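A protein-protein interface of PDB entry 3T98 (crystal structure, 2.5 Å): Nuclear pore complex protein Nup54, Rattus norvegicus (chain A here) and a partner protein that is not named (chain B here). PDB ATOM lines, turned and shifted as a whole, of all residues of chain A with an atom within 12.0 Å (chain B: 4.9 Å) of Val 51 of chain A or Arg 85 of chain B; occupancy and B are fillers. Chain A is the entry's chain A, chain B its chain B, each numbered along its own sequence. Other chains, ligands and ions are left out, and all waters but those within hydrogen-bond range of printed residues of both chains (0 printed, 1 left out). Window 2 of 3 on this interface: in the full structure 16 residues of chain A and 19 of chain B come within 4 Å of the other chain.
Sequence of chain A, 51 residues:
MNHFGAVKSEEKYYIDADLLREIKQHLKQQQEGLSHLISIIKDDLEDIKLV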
ATOM      1  N   ILE A  41      25.328 -25.577  41.781  1.00  0.00           N
ATOM      2  CA  ILE A  41      24.599 -25.304  40.557  1.00  0.00           C
ATOM      3  C   ILE A  41      25.407 -24.380  39.642  1.00  0.00           C
ATOM      4  O   ILE A  41      25.489 -24.611  38.439  1.00  0.00           O
ATOM      5  CB  ILE A  41      23.216 -24.655  40.877  1.00  0.00           C
ATOM      6  CG1 ILE A  41      22.291 -25.708  41.505  1.00  0.00           C
ATOM      7  CG2 ILE A  41      22.582 -24.067  39.604  1.00  0.00           C
ATOM      8  CD1 ILE A  41      21.093 -25.125  42.231  1.00  0.00           C
ATOM      9  N   LYS A  42      26.000 -23.332  40.207  1.00  0.00           N
ATOM     10  CA  LYS A  42      26.791 -22.393  39.405  1.00  0.00           C
ATOM     11  C   LYS A  42      28.002 -23.072  38.768  1.00  0.00           C
ATOM     12  O   LYS A  42      28.364 -22.763  37.636  1.00  0.00           O
ATOM     13  CB  LYS A  42      27.248 -21.212  40.256  1.00  0.00           C
ATOM     14  CG  LYS A  42      26.112 -20.317  40.659  1.00  0.00           C
ATOM     15  CD  LYS A  42      26.547 -19.297  41.669  1.00  0.00           C
ATOM     16  CE  LYS A  42      27.380 -18.207  41.030  1.00  0.00           C
ATOM     17  NZ  LYS A  42      27.637 -17.111  42.006  1.00  0.00           N
ATOM     18  N   ASP A  43      28.628 -23.996  39.488  1.00  0.00           N
ATOM     19  CA  ASP A  43      29.769 -24.709  38.929  1.00  0.00           C
ATOM     20  C   ASP A  43      29.295 -25.516  37.730  1.00  0.00           C
ATOM     21  O   ASP A  43      29.991 -25.592  36.719  1.00  0.00           O
ATOM     22  CB  ASP A  43      30.418 -25.629  39.974  1.00  0.00           C
ATOM     23  CG  ASP A  43      31.258 -24.858  40.988  1.00  0.00           C
ATOM     24  OD1 ASP A  43      31.935 -23.898  40.563  1.00  0.00           O
ATOM     25  OD2 ASP A  43      31.259 -25.211  42.196  1.00  0.00           O
ATOM     26  N   ASP A  44      28.101 -26.096  37.835  1.00  0.00           N
ATOM     27  CA  ASP A  44      27.543 -26.877  36.740  1.00  0.00           C
ATOM     28  C   ASP A  44      27.345 -26.021  35.496  1.00  0.00           C
ATOM     29  O   ASP A  44      27.741 -26.396  34.394  1.00  0.00           O
ATOM     30  CB  ASP A  44      26.196 -27.477  37.131  1.00  0.00           C
ATOM     31  CG  ASP A  44      26.330 -28.665  38.064  1.00  0.00           C
ATOM     32  OD1 ASP A  44      27.186 -29.546  37.806  1.00  0.00           O
ATOM     33  OD2 ASP A  44      25.559 -28.725  39.047  1.00  0.00           O
ATOM     34  N   LEU A  45      26.714 -24.870  35.677  1.00  0.00           N
ATOM     35  CA  LEU A  45      26.472 -23.969  34.560  1.00  0.00           C
ATOM     36  C   LEU A  45      27.793 -23.468  33.985  1.00  0.00           C
ATOM     37  O   LEU A  45      27.956 -23.418  32.769  1.00  0.00           O
ATOM     38  CB  LEU A  45      25.599 -22.784  35.004  1.00  0.00           C
ATOM     39  CG  LEU A  45      24.194 -23.149  35.517  1.00  0.00           C
ATOM     40  CD1 LEU A  45      23.550 -21.937  36.147  1.00  0.00           C
ATOM     41  CD2 LEU A  45      23.336 -23.668  34.377  1.00  0.00           C
ATOM     42  N   GLU A  46      28.739 -23.109  34.842  1.00  0.00           N
ATOM     43  CA  GLU A  46      30.027 -22.619  34.355  1.00  0.00           C
ATOM     44  C   GLU A  46      30.786 -23.710  33.591  1.00  0.00           C
ATOM     45  O   GLU A  46      31.346 -23.460  32.525  1.00  0.00           O
ATOM     46  CB  GLU A  46      30.872 -22.104  35.522  1.00  0.00           C
ATOM     47  CG  GLU A  46      30.179 -20.994  36.282  1.00  0.00           C
ATOM     48  CD  GLU A  46      30.948 -20.552  37.499  1.00  0.00           C
ATOM     49  OE1 GLU A  46      31.555 -21.418  38.172  1.00  0.00           O
ATOM     50  OE2 GLU A  46      30.932 -19.337  37.792  1.00  0.00           O
ATOM     51  N   ASP A  47      30.787 -24.920  34.141  1.00  0.00           N
ATOM     52  CA  ASP A  47      31.450 -26.050  33.510  1.00  0.00           C
ATOM     53  C   ASP A  47      30.790 -26.402  32.170  1.00  0.00           C
ATOM     54  O   ASP A  47      31.428 -26.992  31.299  1.00  0.00           O
ATOM     55  CB  ASP A  47      31.438 -27.254  34.451  1.00  0.00           C
ATOM     56  CG  ASP A  47      32.436 -27.115  35.604  1.00  0.00           C
ATOM     57  OD1 ASP A  47      32.898 -25.979  35.891  1.00  0.00           O
ATOM     58  OD2 ASP A  47      32.754 -28.151  36.235  1.00  0.00           O
ATOM     59  N   ILE A  48      29.521 -26.041  31.997  1.00  0.00           N
ATOM     60  CA  ILE A  48      28.839 -26.306  30.730  1.00  0.00           C
ATOM     61  C   ILE A  48      29.475 -25.429  29.660  1.00  0.00           C
ATOM     62  O   ILE A  48      29.750 -25.888  28.551  1.00  0.00           O
ATOM     63  CB  ILE A  48      27.307 -26.002  30.810  1.00  0.00           C
ATOM     64  CG1 ILE A  48      26.585 -27.153  31.518  1.00  0.00           C
ATOM     65  CG2 ILE A  48      26.719 -25.813  29.409  1.00  0.00           C
ATOM     66  CD1 ILE A  48      25.086 -27.010  31.532  1.00  0.00           C
ATOM     67  N   LYS A  49      29.717 -24.163  30.002  1.00  0.00           N
ATOM     68  CA  LYS A  49      30.328 -23.221  29.069  1.00  0.00           C
ATOM     69  C   LYS A  49      31.774 -23.608  28.767  1.00  0.00           C
ATOM     70  O   LYS A  49      32.322 -23.234  27.736  1.00  0.00           O
ATOM     71  CB  LYS A  49      30.306 -21.808  29.642  1.00  0.00           C
ATOM     72  CG  LYS A  49      30.743 -20.752  28.631  1.00  0.00           C
ATOM     73  CD  LYS A  49      30.572 -19.333  29.166  1.00  0.00           C
ATOM     74  CE  LYS A  49      30.920 -18.295  28.097  1.00  0.00           C
ATOM     75  NZ  LYS A  49      30.062 -18.444  26.880  1.00  0.00           N
ATOM     76  N   LEU A  50      32.379 -24.375  29.665  1.00  0.00           N
ATOM     77  CA  LEU A  50      33.752 -24.804  29.502  1.00  0.00           C
ATOM     78  C   LEU A  50      33.910 -26.116  28.736  1.00  0.00           C
ATOM     79  O   LEU A  50      34.986 -26.408  28.229  1.00  0.00           O
ATOM     80  CB  LEU A  50      34.409 -24.939  30.880  1.00  0.00           C
ATOM     81  CG  LEU A  50      34.557 -23.672  31.736  1.00  0.00           C
ATOM     82  CD1 LEU A  50      35.256 -24.043  33.021  1.00  0.00           C
ATOM     83  CD2 LEU A  50      35.355 -22.600  31.009  1.00  0.00           C
ATOM     84  N   VAL A  51      32.839 -26.896  28.635  1.00  0.00           N
ATOM     85  CA  VAL A  51      32.889 -28.201  27.960  1.00  0.00           C
ATOM     86  C   VAL A  51      32.280 -28.243  26.548  1.00  0.00           C
ATOM     87  O   VAL A  51      31.842 -27.184  26.053  1.00  0.00           O
ATOM     88  CB  VAL A  51      32.192 -29.264  28.842  1.00  0.00           C
ATOM     89  CG1 VAL A  51      30.731 -28.891  29.020  1.00  0.00           C
ATOM     90  CG2 VAL A  51      32.337 -30.657  28.236  1.00  0.00           C
ATOM     91  OXT VAL A  51      32.258 -29.333  25.939  1.00  0.00           O
ATOM     92  N   LYS B  78      23.917 -31.114  30.811  1.00  0.00           N
ATOM     93  CA  LYS B  78      25.300 -31.340  30.436  1.00  0.00           C
ATOM     94  C   LYS B  78      25.520 -32.700  29.775  1.00  0.00           C
ATOM     95  O   LYS B  78      26.134 -32.786  28.710  1.00  0.00           O
ATOM     96  CB  LYS B  78      26.206 -31.210  31.648  1.00  0.00           C
ATOM     97  CG  LYS B  78      27.666 -31.196  31.277  1.00  0.00           C
ATOM     98  CD  LYS B  78      28.517 -31.099  32.518  1.00  0.00           C
ATOM     99  CE  LYS B  78      29.953 -30.782  32.165  1.00  0.00           C
ATOM    100  NZ  LYS B  78      30.804 -30.883  33.374  1.00  0.00           N
ATOM    101  N   TYR B  81      24.018 -32.599  26.332  1.00  0.00           N
ATOM    102  CA  TYR B  81      24.716 -31.645  25.482  1.00  0.00           C
ATOM    103  C   TYR B  81      26.056 -32.275  25.108  1.00  0.00           C
ATOM    104  O   TYR B  81      26.523 -32.164  23.985  1.00  0.00           O
ATOM    105  CB  TYR B  81      24.949 -30.347  26.243  1.00  0.00           C
ATOM    106  CG  TYR B  81      25.959 -29.418  25.606  1.00  0.00           C
ATOM    107  CD1 TYR B  81      25.851 -29.051  24.271  1.00  0.00           C
ATOM    108  CD2 TYR B  81      26.993 -28.861  26.363  1.00  0.00           C
ATOM    109  CE1 TYR B  81      26.743 -28.147  23.697  1.00  0.00           C
ATOM    110  CE2 TYR B  81      27.892 -27.949  25.807  1.00  0.00           C
ATOM    111  CZ  TYR B  81      27.759 -27.592  24.472  1.00  0.00           C
ATOM    112  OH  TYR B  81      28.616 -26.671  23.916  1.00  0.00           O
ATOM    113  N   LEU B  82      26.674 -32.939  26.070  1.00  0.00           N
ATOM    114  CA  LEU B  82      27.940 -33.609  25.821  1.00  0.00           C
ATOM    115  C   LEU B  82      27.769 -34.757  24.817  1.00  0.00           C
ATOM    116  O   LEU B  82      28.632 -34.992  23.962  1.00  0.00           O
ATOM    117  CB  LEU B  82      28.490 -34.165  27.127  1.00  0.00           C
ATOM    118  CG  LEU B  82      29.637 -33.370  27.709  1.00  0.00           C
ATOM    119  CD1 LEU B  82      29.947 -33.877  29.110  1.00  0.00           C
ATOM    120  CD2 LEU B  82      30.845 -33.506  26.784  1.00  0.00           C
ATOM    121  N   SER B  83      26.656 -35.474  24.929  1.00  0.00           N
ATOM    122  CA  SER B  83      26.419 -36.595  24.042  1.00  0.00           C
ATOM    123  C   SER B  83      26.236 -36.107  22.623  1.00  0.00           C
ATOM    124  O   SER B  83      26.865 -36.625  21.683  1.00  0.00           O
ATOM    125  CB  SER B  83      25.206 -37.392  24.514  1.00  0.00           C
ATOM    126  OG  SER B  83      25.512 -38.005  25.760  1.00  0.00           O
ATOM    127  N   TYR B  84      25.387 -35.096  22.469  1.00  0.00           N
ATOM    128  CA  TYR B  84      25.150 -34.523  21.159  1.00  0.00           C
ATOM    129  C   TYR B  84      26.452 -34.039  20.531  1.00  0.00           C
ATOM    130  O   TYR B  84      26.668 -34.199  19.338  1.00  0.00           O
ATOM    131  CB  TYR B  84      24.166 -33.365  21.259  1.00  0.00           C
ATOM    132  CG  TYR B  84      22.743 -33.793  21.442  1.00  0.00           C
ATOM    133  CD1 TYR B  84      22.176 -34.769  20.621  1.00  0.00           C
ATOM    134  CD2 TYR B  84      21.931 -33.178  22.395  1.00  0.00           C
ATOM    135  CE1 TYR B  84      20.838 -35.112  20.739  1.00  0.00           C
ATOM    136  CE2 TYR B  84      20.590 -33.511  22.523  1.00  0.00           C
ATOM    137  CZ  TYR B  84      20.046 -34.477  21.693  1.00  0.00           C
ATOM    138  OH  TYR B  84      18.706 -34.788  21.804  1.00  0.00           O
ATOM    139  N   ARG B  85      27.319 -33.443  21.335  1.00  0.00           N
ATOM    140  CA  ARG B  85      28.585 -32.948  20.821  1.00  0.00           C
ATOM    141  C   ARG B  85      29.437 -34.080  20.260  1.00  0.00           C
ATOM    142  O   ARG B  85      30.059 -33.924  19.213  1.00  0.00           O
ATOM    143  CB  ARG B  85      29.354 -32.222  21.924  1.00  0.00           C
ATOM    144  CG  ARG B  85      28.832 -30.845  22.255  1.00  0.00           C
ATOM    145  CD  ARG B  85      29.690 -30.190  23.319  1.00  0.00           C
ATOM    146  NE  ARG B  85      31.010 -29.839  22.805  1.00  0.00           N
ATOM    147  CZ  ARG B  85      31.273 -28.760  22.073  1.00  0.00           C
ATOM    148  NH1 ARG B  85      30.308 -27.897  21.764  1.00  0.00           N
ATOM    149  NH2 ARG B  85      32.505 -28.553  21.633  1.00  0.00           N
ATOM    150  N   LYS B  86      29.460 -35.217  20.959  1.00  0.00           N
ATOM    151  CA  LYS B  86      30.235 -36.377  20.519  1.00  0.00           C
ATOM    152  C   LYS B  86      29.661 -36.949  19.238  1.00  0.00           C
ATOM    153  O   LYS B  86      30.395 -37.445  18.387  1.00  0.00           O
ATOM    154  CB  LYS B  86      30.255 -37.473  21.586  1.00  0.00           C
ATOM    155  CG  LYS B  86      30.891 -37.057  22.906  1.00  0.00           C
ATOM    156  CD  LYS B  86      31.296 -38.279  23.732  1.00  0.00           C
ATOM    157  CE  LYS B  86      31.813 -37.899  25.121  1.00  0.00           C
ATOM    158  NZ  LYS B  86      30.709 -37.676  26.128  1.00  0.00           N
ATOM    159  N   MET B  87      28.347 -36.869  19.093  1.00  0.00           N
ATOM    160  CA  MET B  87      27.691 -37.392  17.900  1.00  0.00           C
ATOM    161  C   MET B  87      27.912 -36.503  16.685  1.00  0.00           C
ATOM    162  O   MET B  87      28.227 -36.975  15.600  1.00  0.00           O
ATOM    163  CB  MET B  87      26.179 -37.508  18.118  1.00  0.00           C
ATOM    164  CG  MET B  87      25.706 -38.552  19.111  1.00  0.00           C
ATOM    165  SD  MET B  87      23.925 -38.298  19.480  1.00  0.00           S
ATOM    166  CE  MET B  87      23.264 -38.311  17.859  1.00  0.00           C
ATOM    167  N   PHE B  88      27.750 -35.201  16.884  1.00  0.00           N
ATOM    168  CA  PHE B  88      27.847 -34.249  15.787  1.00  0.00           C
ATOM    169  C   PHE B  88      29.118 -33.437  15.591  1.00  0.00           C
ATOM    170  O   PHE B  88      29.369 -32.978  14.485  1.00  0.00           O
ATOM    171  CB  PHE B  88      26.645 -33.301  15.869  1.00  0.00           C
ATOM    172  CG  PHE B  88      25.324 -33.995  15.702  1.00  0.00           C
ATOM    173  CD1 PHE B  88      24.885 -34.393  14.439  1.00  0.00           C
ATOM    174  CD2 PHE B  88      24.532 -34.293  16.811  1.00  0.00           C
ATOM    175  CE1 PHE B  88      23.670 -35.088  14.289  1.00  0.00           C
ATOM    176  CE2 PHE B  88      23.324 -34.984  16.672  1.00  0.00           C
ATOM    177  CZ  PHE B  88      22.890 -35.381  15.411  1.00  0.00           C
ATOM    178  N   LEU B  89      29.927 -33.268  16.628  1.00  0.00           N
ATOM    179  CA  LEU B  89      31.126 -32.444  16.496  1.00  0.00           C
ATOM    180  C   LEU B  89      32.496 -33.137  16.528  1.00  0.00           C
ATOM    181  O   LEU B  89      33.434 -32.686  15.860  1.00  0.00           O
ATOM    182  CB  LEU B  89      31.082 -31.321  17.544  1.00  0.00           C
ATOM    183  CG  LEU B  89      29.873 -30.384  17.425  1.00  0.00           C
ATOM    184  CD1 LEU B  89      29.837 -29.414  18.580  1.00  0.00           C
ATOM    185  CD2 LEU B  89      29.950 -29.632  16.135  1.00  0.00           C
ATOM    186  N   GLY B  90      32.623 -34.220  17.290  1.00  0.00           N
ATOM    187  CA  GLY B  90      33.904 -34.912  17.364  1.00  0.00           C
ATOM    188  C   GLY B  90      34.636 -34.985  16.027  1.00  0.00           C
ATOM    189  O   GLY B  90      35.763 -34.446  15.918  1.00  0.00           O
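Of chain B, only Lys 78 (3.8 Å), Tyr 81 (3.9 Å), Leu 82 (3.5 Å) and Arg 85 (3.4 Å) come within 4 Å of Val 51 of chain A.
Of chain A, only Val 51 comes within 4 Å of Arg 85 of chain B.
Of chain A, only Asp 47 and Val 51 come within 4 Å of Lys 78 of chain B.
Of the printed residues of chain A, Leu 82 of chain B touches Val 51 (3.5 Å).
No residue of chain A comes within 4 Å of Ser 83 of chain B.
No residue of chain A comes within 4 Å of Lys 86 of chain B.
Met 87 of chain B touches none of the printed residues of chain A.
No residue of chain A comes within 4 Å of Leu 89 of chain B.
No residue of chain A comes within 4 Å of Gly 90 of chain B.
Printed residues of chain B within 4 Å of Ile 48 of chain A: Tyr 81.
Of the printed residues of chain B, Asp 47 of chain A touches Lys 78 (3.8 Å).
The nearest printed residue of chain B that does not touch Val 51 of chain A is Lys 86 of chain B (7.5 Å).
The nearest printed residue of chain B that does not touch Ile 48 of chain A is Lys 78 of chain B (4.1 Å).
OH of Tyr 81 of chain B sits at hydrogen-bond distance from NH1 of Arg 85 of chain B, 3.0 Å away.
The backbone NH of Gly 90 of chain B is in hydrogen-bond range of the backbone carbonyl oxygen of Arg 85 of chain B, 3.2 Å away.
Among the printed residues, pairs that only touch across the chains: Val 51 of chain A with Leu 82 of chain B (3.5 Å), Val 51 of chain A with Lys 78 of chain B (3.8 Å), Asp 47 of chain A with Lys 78 of chain B (3.8 Å), Ile 48 of chain A with Tyr 81 of chain B (3.9 Å) and Val 51 of chain A with Tyr 81 of chain B (3.9 Å).
The chain-end carboxylate of Val 51 of chain A is in salt-bridge range of the guanidinium group of Arg 85 of chain B, at 3.4 Å.
Printed residues of chain A that touch a printed residue of chain B: Asp 47, Ile 48 and Val 51.
Of the 11 printed residues of chain B, 4 touch a printed residue of chain A.
Hydrophobic or aromatic side chains of chain B within 4 Å of the printed part of chain A: Tyr 81 and Leu 82.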
